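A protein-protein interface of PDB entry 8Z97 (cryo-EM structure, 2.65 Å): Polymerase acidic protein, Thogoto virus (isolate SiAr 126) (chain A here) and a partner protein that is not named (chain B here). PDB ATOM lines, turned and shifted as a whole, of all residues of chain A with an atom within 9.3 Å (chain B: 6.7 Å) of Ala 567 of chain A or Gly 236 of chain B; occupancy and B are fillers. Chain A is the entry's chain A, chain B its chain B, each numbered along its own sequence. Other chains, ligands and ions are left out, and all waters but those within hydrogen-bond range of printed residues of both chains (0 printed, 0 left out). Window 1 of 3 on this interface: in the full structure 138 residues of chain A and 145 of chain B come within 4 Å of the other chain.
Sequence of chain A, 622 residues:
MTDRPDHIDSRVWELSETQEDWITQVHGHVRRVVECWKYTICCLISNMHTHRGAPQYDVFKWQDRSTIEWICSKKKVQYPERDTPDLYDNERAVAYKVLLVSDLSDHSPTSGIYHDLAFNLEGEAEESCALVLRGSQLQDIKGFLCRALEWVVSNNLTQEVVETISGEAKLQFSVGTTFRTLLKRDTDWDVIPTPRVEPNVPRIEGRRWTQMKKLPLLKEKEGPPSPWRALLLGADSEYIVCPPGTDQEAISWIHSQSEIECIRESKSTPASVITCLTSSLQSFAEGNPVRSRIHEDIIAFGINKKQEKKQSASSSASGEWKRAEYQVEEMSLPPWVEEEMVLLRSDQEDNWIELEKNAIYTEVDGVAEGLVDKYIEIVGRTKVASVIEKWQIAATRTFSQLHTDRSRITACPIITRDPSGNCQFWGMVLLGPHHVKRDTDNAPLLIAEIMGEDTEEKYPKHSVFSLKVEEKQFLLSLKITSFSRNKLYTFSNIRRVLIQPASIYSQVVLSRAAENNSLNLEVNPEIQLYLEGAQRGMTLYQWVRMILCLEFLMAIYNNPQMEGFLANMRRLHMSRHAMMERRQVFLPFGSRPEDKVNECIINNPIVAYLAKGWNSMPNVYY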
ATOM      1  N   MET A 554      24.068   5.434  25.244  1.00  0.00           N
ATOM      2  CA  MET A 554      22.946   4.566  25.580  1.00  0.00           C
ATOM      3  C   MET A 554      23.426   3.230  26.130  1.00  0.00           C
ATOM      4  O   MET A 554      22.838   2.693  27.075  1.00  0.00           O
ATOM      5  CB  MET A 554      22.081   4.356  24.339  1.00  0.00           C
ATOM      6  CG  MET A 554      21.379   5.611  23.859  1.00  0.00           C
ATOM      7  SD  MET A 554      20.443   5.369  22.341  1.00  0.00           S
ATOM      8  CE  MET A 554      19.108   4.357  22.934  1.00  0.00           C
ATOM      9  N   ASN A 558      22.584   1.581  30.159  1.00  0.00           N
ATOM     10  CA  ASN A 558      21.519   0.612  29.943  1.00  0.00           C
ATOM     11  C   ASN A 558      21.032   0.076  31.285  1.00  0.00           C
ATOM     12  O   ASN A 558      21.796  -0.548  32.027  1.00  0.00           O
ATOM     13  CB  ASN A 558      22.007  -0.527  29.053  1.00  0.00           C
ATOM     14  CG  ASN A 558      20.879  -1.408  28.563  1.00  0.00           C
ATOM     15  OD1 ASN A 558      19.711  -1.149  28.841  1.00  0.00           O
ATOM     16  ND2 ASN A 558      21.224  -2.459  27.834  1.00  0.00           N
ATOM     17  N   ASN A 559      19.764   0.322  31.591  1.00  0.00           N
ATOM     18  CA  ASN A 559      19.126  -0.154  32.810  1.00  0.00           C
ATOM     19  C   ASN A 559      17.712  -0.611  32.463  1.00  0.00           C
ATOM     20  O   ASN A 559      17.313  -0.513  31.296  1.00  0.00           O
ATOM     21  CB  ASN A 559      19.131   0.940  33.883  1.00  0.00           C
ATOM     22  CG  ASN A 559      18.588   2.263  33.380  1.00  0.00           C
ATOM     23  OD1 ASN A 559      17.667   2.307  32.566  1.00  0.00           O
ATOM     24  ND2 ASN A 559      19.158   3.354  33.872  1.00  0.00           N
ATOM     25  N   PRO A 560      16.940  -1.144  33.417  1.00  0.00           N
ATOM     26  CA  PRO A 560      15.541  -1.479  33.109  1.00  0.00           C
ATOM     27  C   PRO A 560      14.747  -0.328  32.513  1.00  0.00           C
ATOM     28  O   PRO A 560      13.929  -0.555  31.613  1.00  0.00           O
ATOM     29  CB  PRO A 560      14.974  -1.900  34.472  1.00  0.00           C
ATOM     30  CG  PRO A 560      16.156  -2.226  35.329  1.00  0.00           C
ATOM     31  CD  PRO A 560      17.416  -1.862  34.609  1.00  0.00           C
ATOM     32  N   GLN A 561      14.962   0.901  32.987  1.00  0.00           N
ATOM     33  CA  GLN A 561      14.248   2.041  32.420  1.00  0.00           C
ATOM     34  C   GLN A 561      14.600   2.231  30.951  1.00  0.00           C
ATOM     35  O   GLN A 561      13.716   2.423  30.110  1.00  0.00           O
ATOM     36  CB  GLN A 561      14.557   3.309  33.215  1.00  0.00           C
ATOM     37  CG  GLN A 561      14.545   3.121  34.715  1.00  0.00           C
ATOM     38  CD  GLN A 561      14.871   4.397  35.457  1.00  0.00           C
ATOM     39  OE1 GLN A 561      14.737   5.493  34.918  1.00  0.00           O
ATOM     40  NE2 GLN A 561      15.306   4.261  36.702  1.00  0.00           N
ATOM     41  N   MET A 562      15.892   2.169  30.620  1.00  0.00           N
ATOM     42  CA  MET A 562      16.307   2.315  29.228  1.00  0.00           C
ATOM     43  C   MET A 562      15.765   1.181  28.369  1.00  0.00           C
ATOM     44  O   MET A 562      15.297   1.409  27.248  1.00  0.00           O
ATOM     45  CB  MET A 562      17.832   2.377  29.141  1.00  0.00           C
ATOM     46  CG  MET A 562      18.382   2.283  27.728  1.00  0.00           C
ATOM     47  SD  MET A 562      18.390   3.865  26.862  1.00  0.00           S
ATOM     48  CE  MET A 562      19.513   4.807  27.889  1.00  0.00           C
ATOM     49  N   GLU A 563      15.814  -0.050  28.884  1.00  0.00           N
ATOM     50  CA  GLU A 563      15.316  -1.196  28.129  1.00  0.00           C
ATOM     51  C   GLU A 563      13.829  -1.049  27.831  1.00  0.00           C
ATOM     52  O   GLU A 563      13.394  -1.219  26.685  1.00  0.00           O
ATOM     53  CB  GLU A 563      15.585  -2.486  28.904  1.00  0.00           C
ATOM     54  CG  GLU A 563      16.964  -3.077  28.675  1.00  0.00           C
ATOM     55  CD  GLU A 563      17.153  -3.592  27.261  1.00  0.00           C
ATOM     56  OE1 GLU A 563      16.159  -4.035  26.652  1.00  0.00           O
ATOM     57  OE2 GLU A 563      18.296  -3.556  26.761  1.00  0.00           O
ATOM     58  N   GLY A 564      13.035  -0.722  28.853  1.00  0.00           N
ATOM     59  CA  GLY A 564      11.608  -0.551  28.641  1.00  0.00           C
ATOM     60  C   GLY A 564      11.285   0.614  27.727  1.00  0.00           C
ATOM     61  O   GLY A 564      10.406   0.514  26.866  1.00  0.00           O
ATOM     62  N   PHE A 565      11.994   1.732  27.896  1.00  0.00           N
ATOM     63  CA  PHE A 565      11.760   2.901  27.057  1.00  0.00           C
ATOM     64  C   PHE A 565      12.041   2.584  25.595  1.00  0.00           C
ATOM     65  O   PHE A 565      11.247   2.922  24.712  1.00  0.00           O
ATOM     66  CB  PHE A 565      12.628   4.063  27.543  1.00  0.00           C
ATOM     67  CG  PHE A 565      12.568   5.282  26.667  1.00  0.00           C
ATOM     68  CD1 PHE A 565      11.587   6.236  26.857  1.00  0.00           C
ATOM     69  CD2 PHE A 565      13.505   5.483  25.667  1.00  0.00           C
ATOM     70  CE1 PHE A 565      11.531   7.359  26.060  1.00  0.00           C
ATOM     71  CE2 PHE A 565      13.453   6.605  24.867  1.00  0.00           C
ATOM     72  CZ  PHE A 565      12.465   7.544  25.064  1.00  0.00           C
ATOM     73  N   LEU A 566      13.164   1.919  25.322  1.00  0.00           N
ATOM     74  CA  LEU A 566      13.492   1.570  23.945  1.00  0.00           C
ATOM     75  C   LEU A 566      12.507   0.561  23.378  1.00  0.00           C
ATOM     76  O   LEU A 566      12.108   0.666  22.213  1.00  0.00           O
ATOM     77  CB  LEU A 566      14.915   1.027  23.865  1.00  0.00           C
ATOM     78  CG  LEU A 566      16.022   2.072  23.905  1.00  0.00           C
ATOM     79  CD1 LEU A 566      17.307   1.434  23.452  1.00  0.00           C
ATOM     80  CD2 LEU A 566      15.666   3.262  23.033  1.00  0.00           C
ATOM     81  N   ALA A 567      12.106  -0.427  24.181  1.00  0.00           N
ATOM     82  CA  ALA A 567      11.178  -1.438  23.690  1.00  0.00           C
ATOM     83  C   ALA A 567       9.824  -0.829  23.356  1.00  0.00           C
ATOM     84  O   ALA A 567       9.177  -1.234  22.383  1.00  0.00           O
ATOM     85  CB  ALA A 567      11.026  -2.554  24.721  1.00  0.00           C
ATOM     86  N   ASN A 568       9.376   0.145  24.147  1.00  0.00           N
ATOM     87  CA  ASN A 568       8.059   0.728  23.941  1.00  0.00           C
ATOM     88  C   ASN A 568       8.064   1.949  23.028  1.00  0.00           C
ATOM     89  O   ASN A 568       6.986   2.398  22.627  1.00  0.00           O
ATOM     90  CB  ASN A 568       7.438   1.096  25.289  1.00  0.00           C
ATOM     91  CG  ASN A 568       7.031  -0.122  26.087  1.00  0.00           C
ATOM     92  OD1 ASN A 568       6.053  -0.792  25.758  1.00  0.00           O
ATOM     93  ND2 ASN A 568       7.784  -0.421  27.135  1.00  0.00           N
ATOM     94  N   MET A 569       9.229   2.496  22.688  1.00  0.00           N
ATOM     95  CA  MET A 569       9.283   3.616  21.757  1.00  0.00           C
ATOM     96  C   MET A 569       9.319   3.183  20.300  1.00  0.00           C
ATOM     97  O   MET A 569       9.174   4.034  19.417  1.00  0.00           O
ATOM     98  CB  MET A 569      10.504   4.494  22.048  1.00  0.00           C
ATOM     99  CG  MET A 569      10.267   5.550  23.110  1.00  0.00           C
ATOM    100  SD  MET A 569       9.161   6.867  22.572  1.00  0.00           S
ATOM    101  CE  MET A 569       9.791   7.188  20.931  1.00  0.00           C
ATOM    102  N   ARG A 570       9.510   1.893  20.026  1.00  0.00           N
ATOM    103  CA  ARG A 570       9.525   1.426  18.645  1.00  0.00           C
ATOM    104  C   ARG A 570       8.150   1.557  18.002  1.00  0.00           C
ATOM    105  O   ARG A 570       8.045   1.878  16.814  1.00  0.00           O
ATOM    106  CB  ARG A 570      10.030  -0.013  18.593  1.00  0.00           C
ATOM    107  CG  ARG A 570      11.436  -0.158  19.141  1.00  0.00           C
ATOM    108  CD  ARG A 570      11.788  -1.593  19.476  1.00  0.00           C
ATOM    109  NE  ARG A 570      13.000  -1.650  20.285  1.00  0.00           N
ATOM    110  CZ  ARG A 570      13.418  -2.724  20.941  1.00  0.00           C
ATOM    111  NH1 ARG A 570      12.743  -3.860  20.906  1.00  0.00           N
ATOM    112  NH2 ARG A 570      14.536  -2.653  21.655  1.00  0.00           N
ATOM    113  N   ARG A 571       7.085   1.327  18.772  1.00  0.00           N
ATOM    114  CA  ARG A 571       5.738   1.530  18.248  1.00  0.00           C
ATOM    115  C   ARG A 571       5.503   2.986  17.874  1.00  0.00           C
ATOM    116  O   ARG A 571       4.918   3.280  16.826  1.00  0.00           O
ATOM    117  CB  ARG A 571       4.701   1.070  19.270  1.00  0.00           C
ATOM    118  CG  ARG A 571       4.272  -0.372  19.111  1.00  0.00           C
ATOM    119  CD  ARG A 571       3.300  -0.773  20.204  1.00  0.00           C
ATOM    120  NE  ARG A 571       3.730  -0.293  21.510  1.00  0.00           N
ATOM    121  CZ  ARG A 571       4.358  -1.034  22.411  1.00  0.00           C
ATOM    122  NH1 ARG A 571       4.647  -2.304  22.180  1.00  0.00           N
ATOM    123  NH2 ARG A 571       4.706  -0.487  23.572  1.00  0.00           N
ATOM    124  N   LEU A 572       5.950   3.915  18.721  1.00  0.00           N
ATOM    125  CA  LEU A 572       5.777   5.333  18.420  1.00  0.00           C
ATOM    126  C   LEU A 572       6.638   5.756  17.237  1.00  0.00           C
ATOM    127  O   LEU A 572       6.223   6.592  16.428  1.00  0.00           O
ATOM    128  CB  LEU A 572       6.098   6.170  19.656  1.00  0.00           C
ATOM    129  CG  LEU A 572       5.109   6.017  20.813  1.00  0.00           C
ATOM    130  CD1 LEU A 572       5.511   6.894  21.984  1.00  0.00           C
ATOM    131  CD2 LEU A 572       3.696   6.337  20.356  1.00  0.00           C
ATOM    132  N   HIS A 573       7.841   5.190  17.122  1.00  0.00           N
ATOM    133  CA  HIS A 573       8.685   5.457  15.961  1.00  0.00           C
ATOM    134  C   HIS A 573       8.020   4.973  14.678  1.00  0.00           C
ATOM    135  O   HIS A 573       8.032   5.671  13.655  1.00  0.00           O
ATOM    136  CB  HIS A 573      10.045   4.788  16.161  1.00  0.00           C
ATOM    137  CG  HIS A 573      11.133   5.338  15.295  1.00  0.00           C
ATOM    138  ND1 HIS A 573      12.017   6.300  15.735  1.00  0.00           N
ATOM    139  CD2 HIS A 573      11.503   5.039  14.028  1.00  0.00           C
ATOM    140  CE1 HIS A 573      12.871   6.584  14.769  1.00  0.00           C
ATOM    141  NE2 HIS A 573      12.583   5.832  13.724  1.00  0.00           N
ATOM    142  N   PRO A 593      -0.616   4.868  24.037  1.00  0.00           N
ATOM    143  CA  PRO A 593       0.726   4.276  23.901  1.00  0.00           C
ATOM    144  C   PRO A 593       1.818   5.049  24.618  1.00  0.00           C
ATOM    145  O   PRO A 593       2.871   4.471  24.910  1.00  0.00           O
ATOM    146  CB  PRO A 593       0.954   4.270  22.383  1.00  0.00           C
ATOM    147  CG  PRO A 593      -0.415   4.342  21.790  1.00  0.00           C
ATOM    148  CD  PRO A 593      -1.207   5.193  22.730  1.00  0.00           C
ATOM    149  N   LYS A 596       2.763   3.678  28.410  1.00  0.00           N
ATOM    150  CA  LYS A 596       3.713   2.579  28.495  1.00  0.00           C
ATOM    151  C   LYS A 596       5.144   3.039  28.253  1.00  0.00           C
ATOM    152  O   LYS A 596       6.083   2.315  28.599  1.00  0.00           O
ATOM    153  CB  LYS A 596       3.330   1.484  27.502  1.00  0.00           C
ATOM    154  CG  LYS A 596       2.043   0.769  27.872  1.00  0.00           C
ATOM    155  CD  LYS A 596       2.025  -0.650  27.353  1.00  0.00           C
ATOM    156  CE  LYS A 596       0.619  -1.220  27.371  1.00  0.00           C
ATOM    157  NZ  LYS A 596       0.017  -1.156  28.730  1.00  0.00           N
ATOM    158  N   VAL A 597       5.326   4.218  27.665  1.00  0.00           N
ATOM    159  CA  VAL A 597       6.649   4.814  27.535  1.00  0.00           C
ATOM    160  C   VAL A 597       6.929   5.777  28.682  1.00  0.00           C
ATOM    161  O   VAL A 597       8.061   5.863  29.165  1.00  0.00           O
ATOM    162  CB  VAL A 597       6.780   5.514  26.169  1.00  0.00           C
ATOM    163  CG1 VAL A 597       8.170   6.089  26.000  1.00  0.00           C
ATOM    164  CG2 VAL A 597       6.459   4.550  25.045  1.00  0.00           C
ATOM    165  N   GLU A 599       5.961   5.513  31.720  1.00  0.00           N
ATOM    166  CA  GLU A 599       6.287   4.772  32.932  1.00  0.00           C
ATOM    167  C   GLU A 599       7.773   4.456  33.036  1.00  0.00           C
ATOM    168  O   GLU A 599       8.274   4.236  34.144  1.00  0.00           O
ATOM    169  CB  GLU A 599       5.476   3.477  32.995  1.00  0.00           C
ATOM    170  CG  GLU A 599       5.814   2.480  31.903  1.00  0.00           C
ATOM    171  CD  GLU A 599       4.948   1.238  31.957  1.00  0.00           C
ATOM    172  OE1 GLU A 599       4.065   1.166  32.837  1.00  0.00           O
ATOM    173  OE2 GLU A 599       5.150   0.333  31.120  1.00  0.00           O
ATOM    174  N   CYS A 600       8.488   4.430  31.913  1.00  0.00           N
ATOM    175  CA  CYS A 600       9.905   4.098  31.898  1.00  0.00           C
ATOM    176  C   CYS A 600      10.812   5.315  32.028  1.00  0.00           C
ATOM    177  O   CYS A 600      12.033   5.148  32.118  1.00  0.00           O
ATOM    178  CB  CYS A 600      10.251   3.342  30.612  1.00  0.00           C
ATOM    179  SG  CYS A 600       9.451   1.730  30.467  1.00  0.00           S
ATOM    180  N   VAL A 607      17.571   8.551  28.704  1.00  0.00           N
ATOM    181  CA  VAL A 607      16.152   8.371  28.408  1.00  0.00           C
ATOM    182  C   VAL A 607      15.454   9.724  28.338  1.00  0.00           C
ATOM    183  O   VAL A 607      14.642   9.975  27.441  1.00  0.00           O
ATOM    184  CB  VAL A 607      15.498   7.440  29.446  1.00  0.00           C
ATOM    185  CG1 VAL A 607      13.988   7.441  29.285  1.00  0.00           C
ATOM    186  CG2 VAL A 607      16.042   6.034  29.300  1.00  0.00           C
ATOM    187  N   LEU A 610      16.461  11.409  25.063  1.00  0.00           N
ATOM    188  CA  LEU A 610      15.698  10.874  23.941  1.00  0.00           C
ATOM    189  C   LEU A 610      14.260  11.374  23.971  1.00  0.00           C
ATOM    190  O   LEU A 610      13.675  11.669  22.923  1.00  0.00           O
ATOM    191  CB  LEU A 610      15.742   9.348  23.964  1.00  0.00           C
ATOM    192  CG  LEU A 610      17.092   8.704  23.642  1.00  0.00           C
ATOM    193  CD1 LEU A 610      17.076   7.228  23.988  1.00  0.00           C
ATOM    194  CD2 LEU A 610      17.454   8.906  22.181  1.00  0.00           C
ATOM    195  N   LEU B  19      17.254   1.746  17.970  1.00  0.00           N
ATOM    196  CA  LEU B  19      16.485   1.730  19.213  1.00  0.00           C
ATOM    197  C   LEU B  19      16.729   0.446  19.994  1.00  0.00           C
ATOM    198  O   LEU B  19      15.802  -0.241  20.417  1.00  0.00           O
ATOM    199  CB  LEU B  19      15.003   1.912  18.909  1.00  0.00           C
ATOM    200  CG  LEU B  19      14.643   3.161  18.106  1.00  0.00           C
ATOM    201  CD1 LEU B  19      13.145   3.240  17.875  1.00  0.00           C
ATOM    202  CD2 LEU B  19      15.145   4.398  18.820  1.00  0.00           C
ATOM    203  N   TYR B  22      21.281  -2.945  23.350  1.00  0.00           N
ATOM    204  CA  TYR B  22      22.082  -4.149  23.481  1.00  0.00           C
ATOM    205  C   TYR B  22      23.558  -3.786  23.325  1.00  0.00           C
ATOM    206  O   TYR B  22      23.912  -2.688  22.888  1.00  0.00           O
ATOM    207  CB  TYR B  22      21.652  -5.201  22.456  1.00  0.00           C
ATOM    208  CG  TYR B  22      20.210  -5.680  22.581  1.00  0.00           C
ATOM    209  CD1 TYR B  22      19.350  -5.156  23.539  1.00  0.00           C
ATOM    210  CD2 TYR B  22      19.715  -6.662  21.738  1.00  0.00           C
ATOM    211  CE1 TYR B  22      18.043  -5.592  23.643  1.00  0.00           C
ATOM    212  CE2 TYR B  22      18.412  -7.104  21.834  1.00  0.00           C
ATOM    213  CZ  TYR B  22      17.581  -6.568  22.788  1.00  0.00           C
ATOM    214  OH  TYR B  22      16.282  -7.010  22.885  1.00  0.00           O
ATOM    215  N   PRO B  27      19.183  -6.208  32.556  1.00  0.00           N
ATOM    216  CA  PRO B  27      18.687  -6.131  33.933  1.00  0.00           C
ATOM    217  C   PRO B  27      18.517  -7.506  34.557  1.00  0.00           C
ATOM    218  O   PRO B  27      18.256  -8.500  33.875  1.00  0.00           O
ATOM    219  CB  PRO B  27      17.338  -5.420  33.784  1.00  0.00           C
ATOM    220  CG  PRO B  27      16.917  -5.710  32.391  1.00  0.00           C
ATOM    221  CD  PRO B  27      18.176  -5.764  31.579  1.00  0.00           C
ATOM    222  N   GLU B 234      16.731 -10.640  31.114  1.00  0.00           N
ATOM    223  CA  GLU B 234      15.657 -10.403  30.159  1.00  0.00           C
ATOM    224  C   GLU B 234      15.655  -8.936  29.756  1.00  0.00           C
ATOM    225  O   GLU B 234      15.688  -8.051  30.617  1.00  0.00           O
ATOM    226  CB  GLU B 234      14.301 -10.797  30.743  1.00  0.00           C
ATOM    227  CG  GLU B 234      13.120 -10.282  29.939  1.00  0.00           C
ATOM    228  CD  GLU B 234      11.813 -10.924  30.346  1.00  0.00           C
ATOM    229  OE1 GLU B 234      11.774 -12.162  30.475  1.00  0.00           O
ATOM    230  OE2 GLU B 234      10.825 -10.192  30.548  1.00  0.00           O
ATOM    231  N   ARG B 235      15.609  -8.684  28.453  1.00  0.00           N
ATOM    232  CA  ARG B 235      15.690  -7.341  27.904  1.00  0.00           C
ATOM    233  C   ARG B 235      14.352  -6.933  27.305  1.00  0.00           C
ATOM    234  O   ARG B 235      13.601  -7.767  26.793  1.00  0.00           O
ATOM    235  CB  ARG B 235      16.787  -7.256  26.838  1.00  0.00           C
ATOM    236  CG  ARG B 235      18.104  -7.883  27.263  1.00  0.00           C
ATOM    237  CD  ARG B 235      19.155  -7.756  26.177  1.00  0.00           C
ATOM    238  NE  ARG B 235      19.976  -6.565  26.354  1.00  0.00           N
ATOM    239  CZ  ARG B 235      21.284  -6.581  26.566  1.00  0.00           C
ATOM    240  NH1 ARG B 235      21.960  -7.715  26.632  1.00  0.00           N
ATOM    241  NH2 ARG B 235      21.930  -5.429  26.715  1.00  0.00           N
ATOM    242  N   GLY B 236      14.057  -5.640  27.383  1.00  0.00           N
ATOM    243  CA  GLY B 236      12.862  -5.089  26.786  1.00  0.00           C
ATOM    244  C   GLY B 236      11.699  -4.849  27.720  1.00  0.00           C
ATOM    245  O   GLY B 236      10.610  -4.509  27.243  1.00  0.00           O
ATOM    246  N   ARG B 237      11.882  -5.020  29.028  1.00  0.00           N
ATOM    247  CA  ARG B 237      10.822  -4.759  29.989  1.00  0.00           C
ATOM    248  C   ARG B 237      11.382  -4.026  31.197  1.00  0.00           C
ATOM    249  O   ARG B 237      12.494  -4.314  31.651  1.00  0.00           O
ATOM    250  CB  ARG B 237      10.127  -6.051  30.439  1.00  0.00           C
ATOM    251  CG  ARG B 237       9.346  -6.748  29.339  1.00  0.00           C
ATOM    252  CD  ARG B 237       8.727  -8.042  29.831  1.00  0.00           C
ATOM    253  NE  ARG B 237       7.725  -7.811  30.864  1.00  0.00           N
ATOM    254  CZ  ARG B 237       6.444  -7.570  30.625  1.00  0.00           C
ATOM    255  NH1 ARG B 237       5.970  -7.516  29.391  1.00  0.00           N
ATOM    256  NH2 ARG B 237       5.618  -7.379  31.649  1.00  0.00           N
ATOM    257  N   LEU B 238      10.600  -3.075  31.708  1.00  0.00           N
ATOM    258  CA  LEU B 238      11.001  -2.338  32.901  1.00  0.00           C
ATOM    259  C   LEU B 238      10.850  -3.179  34.162  1.00  0.00           C
ATOM    260  O   LEU B 238      11.652  -3.046  35.094  1.00  0.00           O
ATOM    261  CB  LEU B 238      10.179  -1.054  33.014  1.00  0.00           C
ATOM    262  CG  LEU B 238      10.253  -0.264  34.323  1.00  0.00           C
ATOM    263  CD1 LEU B 238      11.634   0.336  34.514  1.00  0.00           C
ATOM    264  CD2 LEU B 238       9.186   0.815  34.354  1.00  0.00           C
ATOM    265  N   ARG B 240      10.609  -6.801  36.259  1.00  0.00           N
ATOM    266  CA  ARG B 240      11.004  -8.202  36.245  1.00  0.00           C
ATOM    267  C   ARG B 240       9.781  -9.099  36.383  1.00  0.00           C
ATOM    268  O   ARG B 240       8.845  -8.789  37.125  1.00  0.00           O
ATOM    269  CB  ARG B 240      11.995  -8.490  37.372  1.00  0.00           C
ATOM    270  CG  ARG B 240      13.112  -7.471  37.507  1.00  0.00           C
ATOM    271  CD  ARG B 240      14.222  -7.696  36.488  1.00  0.00           C
ATOM    272  NE  ARG B 240      13.879  -7.194  35.163  1.00  0.00           N
ATOM    273  CZ  ARG B 240      13.753  -5.911  34.850  1.00  0.00           C
ATOM    274  NH1 ARG B 240      13.943  -4.957  35.745  1.00  0.00           N
ATOM    275  NH2 ARG B 240      13.426  -5.578  33.605  1.00  0.00           N
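Of chain B, only Gly 236 comes within 4 Å of Ala 567 of chain A.
Printed residues of chain B within 4 Å of Leu 566 of chain A: Leu 19.
Printed residues of chain B within 4 Å of Asn 558 of chain A: Arg 235 (3.3 Å).
Of the printed residues of chain B, Glu 563 of chain A touches Tyr 22, Arg 235 and Gly 236.
Printed residues of chain B within 4 Å of His 573 of chain A: Leu 19 (3.9 Å).
Printed residues of chain B within 4 Å of Glu 599 of chain A: Leu 238 (3.5 Å).
Glu 234 of chain B touches none of the printed residues of chain A.
The nearest residue of chain A that does not touch Gly 236 of chain B is Gly 564 of chain A (4.3 Å).
Among the printed residues, pairs that only touch across the chains: Ala 567 of chain A with Gly 236 of chain B, Pro 560 of chain A with Arg 240 of chain B, Glu 599 of chain A with Leu 238 of chain B, Pro 560 of chain A with Leu 238 of chain B, Leu 566 of chain A with Leu 19 of chain B, Pro 560 of chain A with Pro 27 of chain B, Gln 561 of chain A with Leu 238 of chain B, Glu 563 of chain A with Tyr 22 of chain B, Cys 600 of chain A with Leu 238 of chain B and His 573 of chain A with Leu 19 of chain B.
The side-chain amide nitrogen (ND2) of Asn 558 of chain A lies within hydrogen-bond range of the side-chain carboxylate (OE2) of Glu 563 of chain A.
OD1 of Asn 559 of chain A sits at hydrogen-bond distance from N of Gln 561 of chain A, at 3.1 Å.
The backbone NH (N) of Phe 565 of chain A lies close to the side-chain sulfur (SG) of Cys 600 of chain A, at 3.6 Å.
The backbone carbonyl oxygen (O) of Leu 566 of chain A lies within hydrogen-bond range of the guanidinium group (NE) of Arg 570 of chain A.
The guanidinium group (NH2) of Arg 240 of chain B sits at hydrogen-bond distance from the backbone carbonyl oxygen (O) of Arg 237 of chain B, at 2.5 Å.
The backbone carbonyl oxygen (O) of Leu 238 of chain B sits at hydrogen-bond distance from the guanidinium group (NH1) of Arg 240 of chain B.
ND2 of Asn 558 of chain A lies close to NH2 of Arg 235 of chain B.
OE2 of Glu 563 of chain A lies within salt-bridge range of NE of Arg 235 of chain B, 3.5 Å away.
N of Gly 236 of chain B is in hydrogen-bond range of OE1 of Glu 563 of chain A (2.7 Å).
The guanidinium group (NH2) of Arg 570 of chain A is in hydrogen-bond range of the backbone carbonyl oxygen (O) of Leu 19 of chain B (3.0 Å).
Hydrophobic or aromatic side chains of chain A that line the printed part of chain B: Pro 560, Leu 566, Ala 567 and His 573.
Of the 9 printed residues of chain B, 7 touch a printed residue of chain A.
Printed residues of chain B that touch a printed residue of chain A: Leu 19, Tyr 22, Pro 27, Arg 235, Gly 236, Leu 238 and Arg 240.
Among the printed residues, Asp or Glu carboxylates within 4 Å of a Lys or Arg side-chain nitrogen of the other chain: Glu 563 of chain A with Arg 235 of chain B (3.5 Å).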
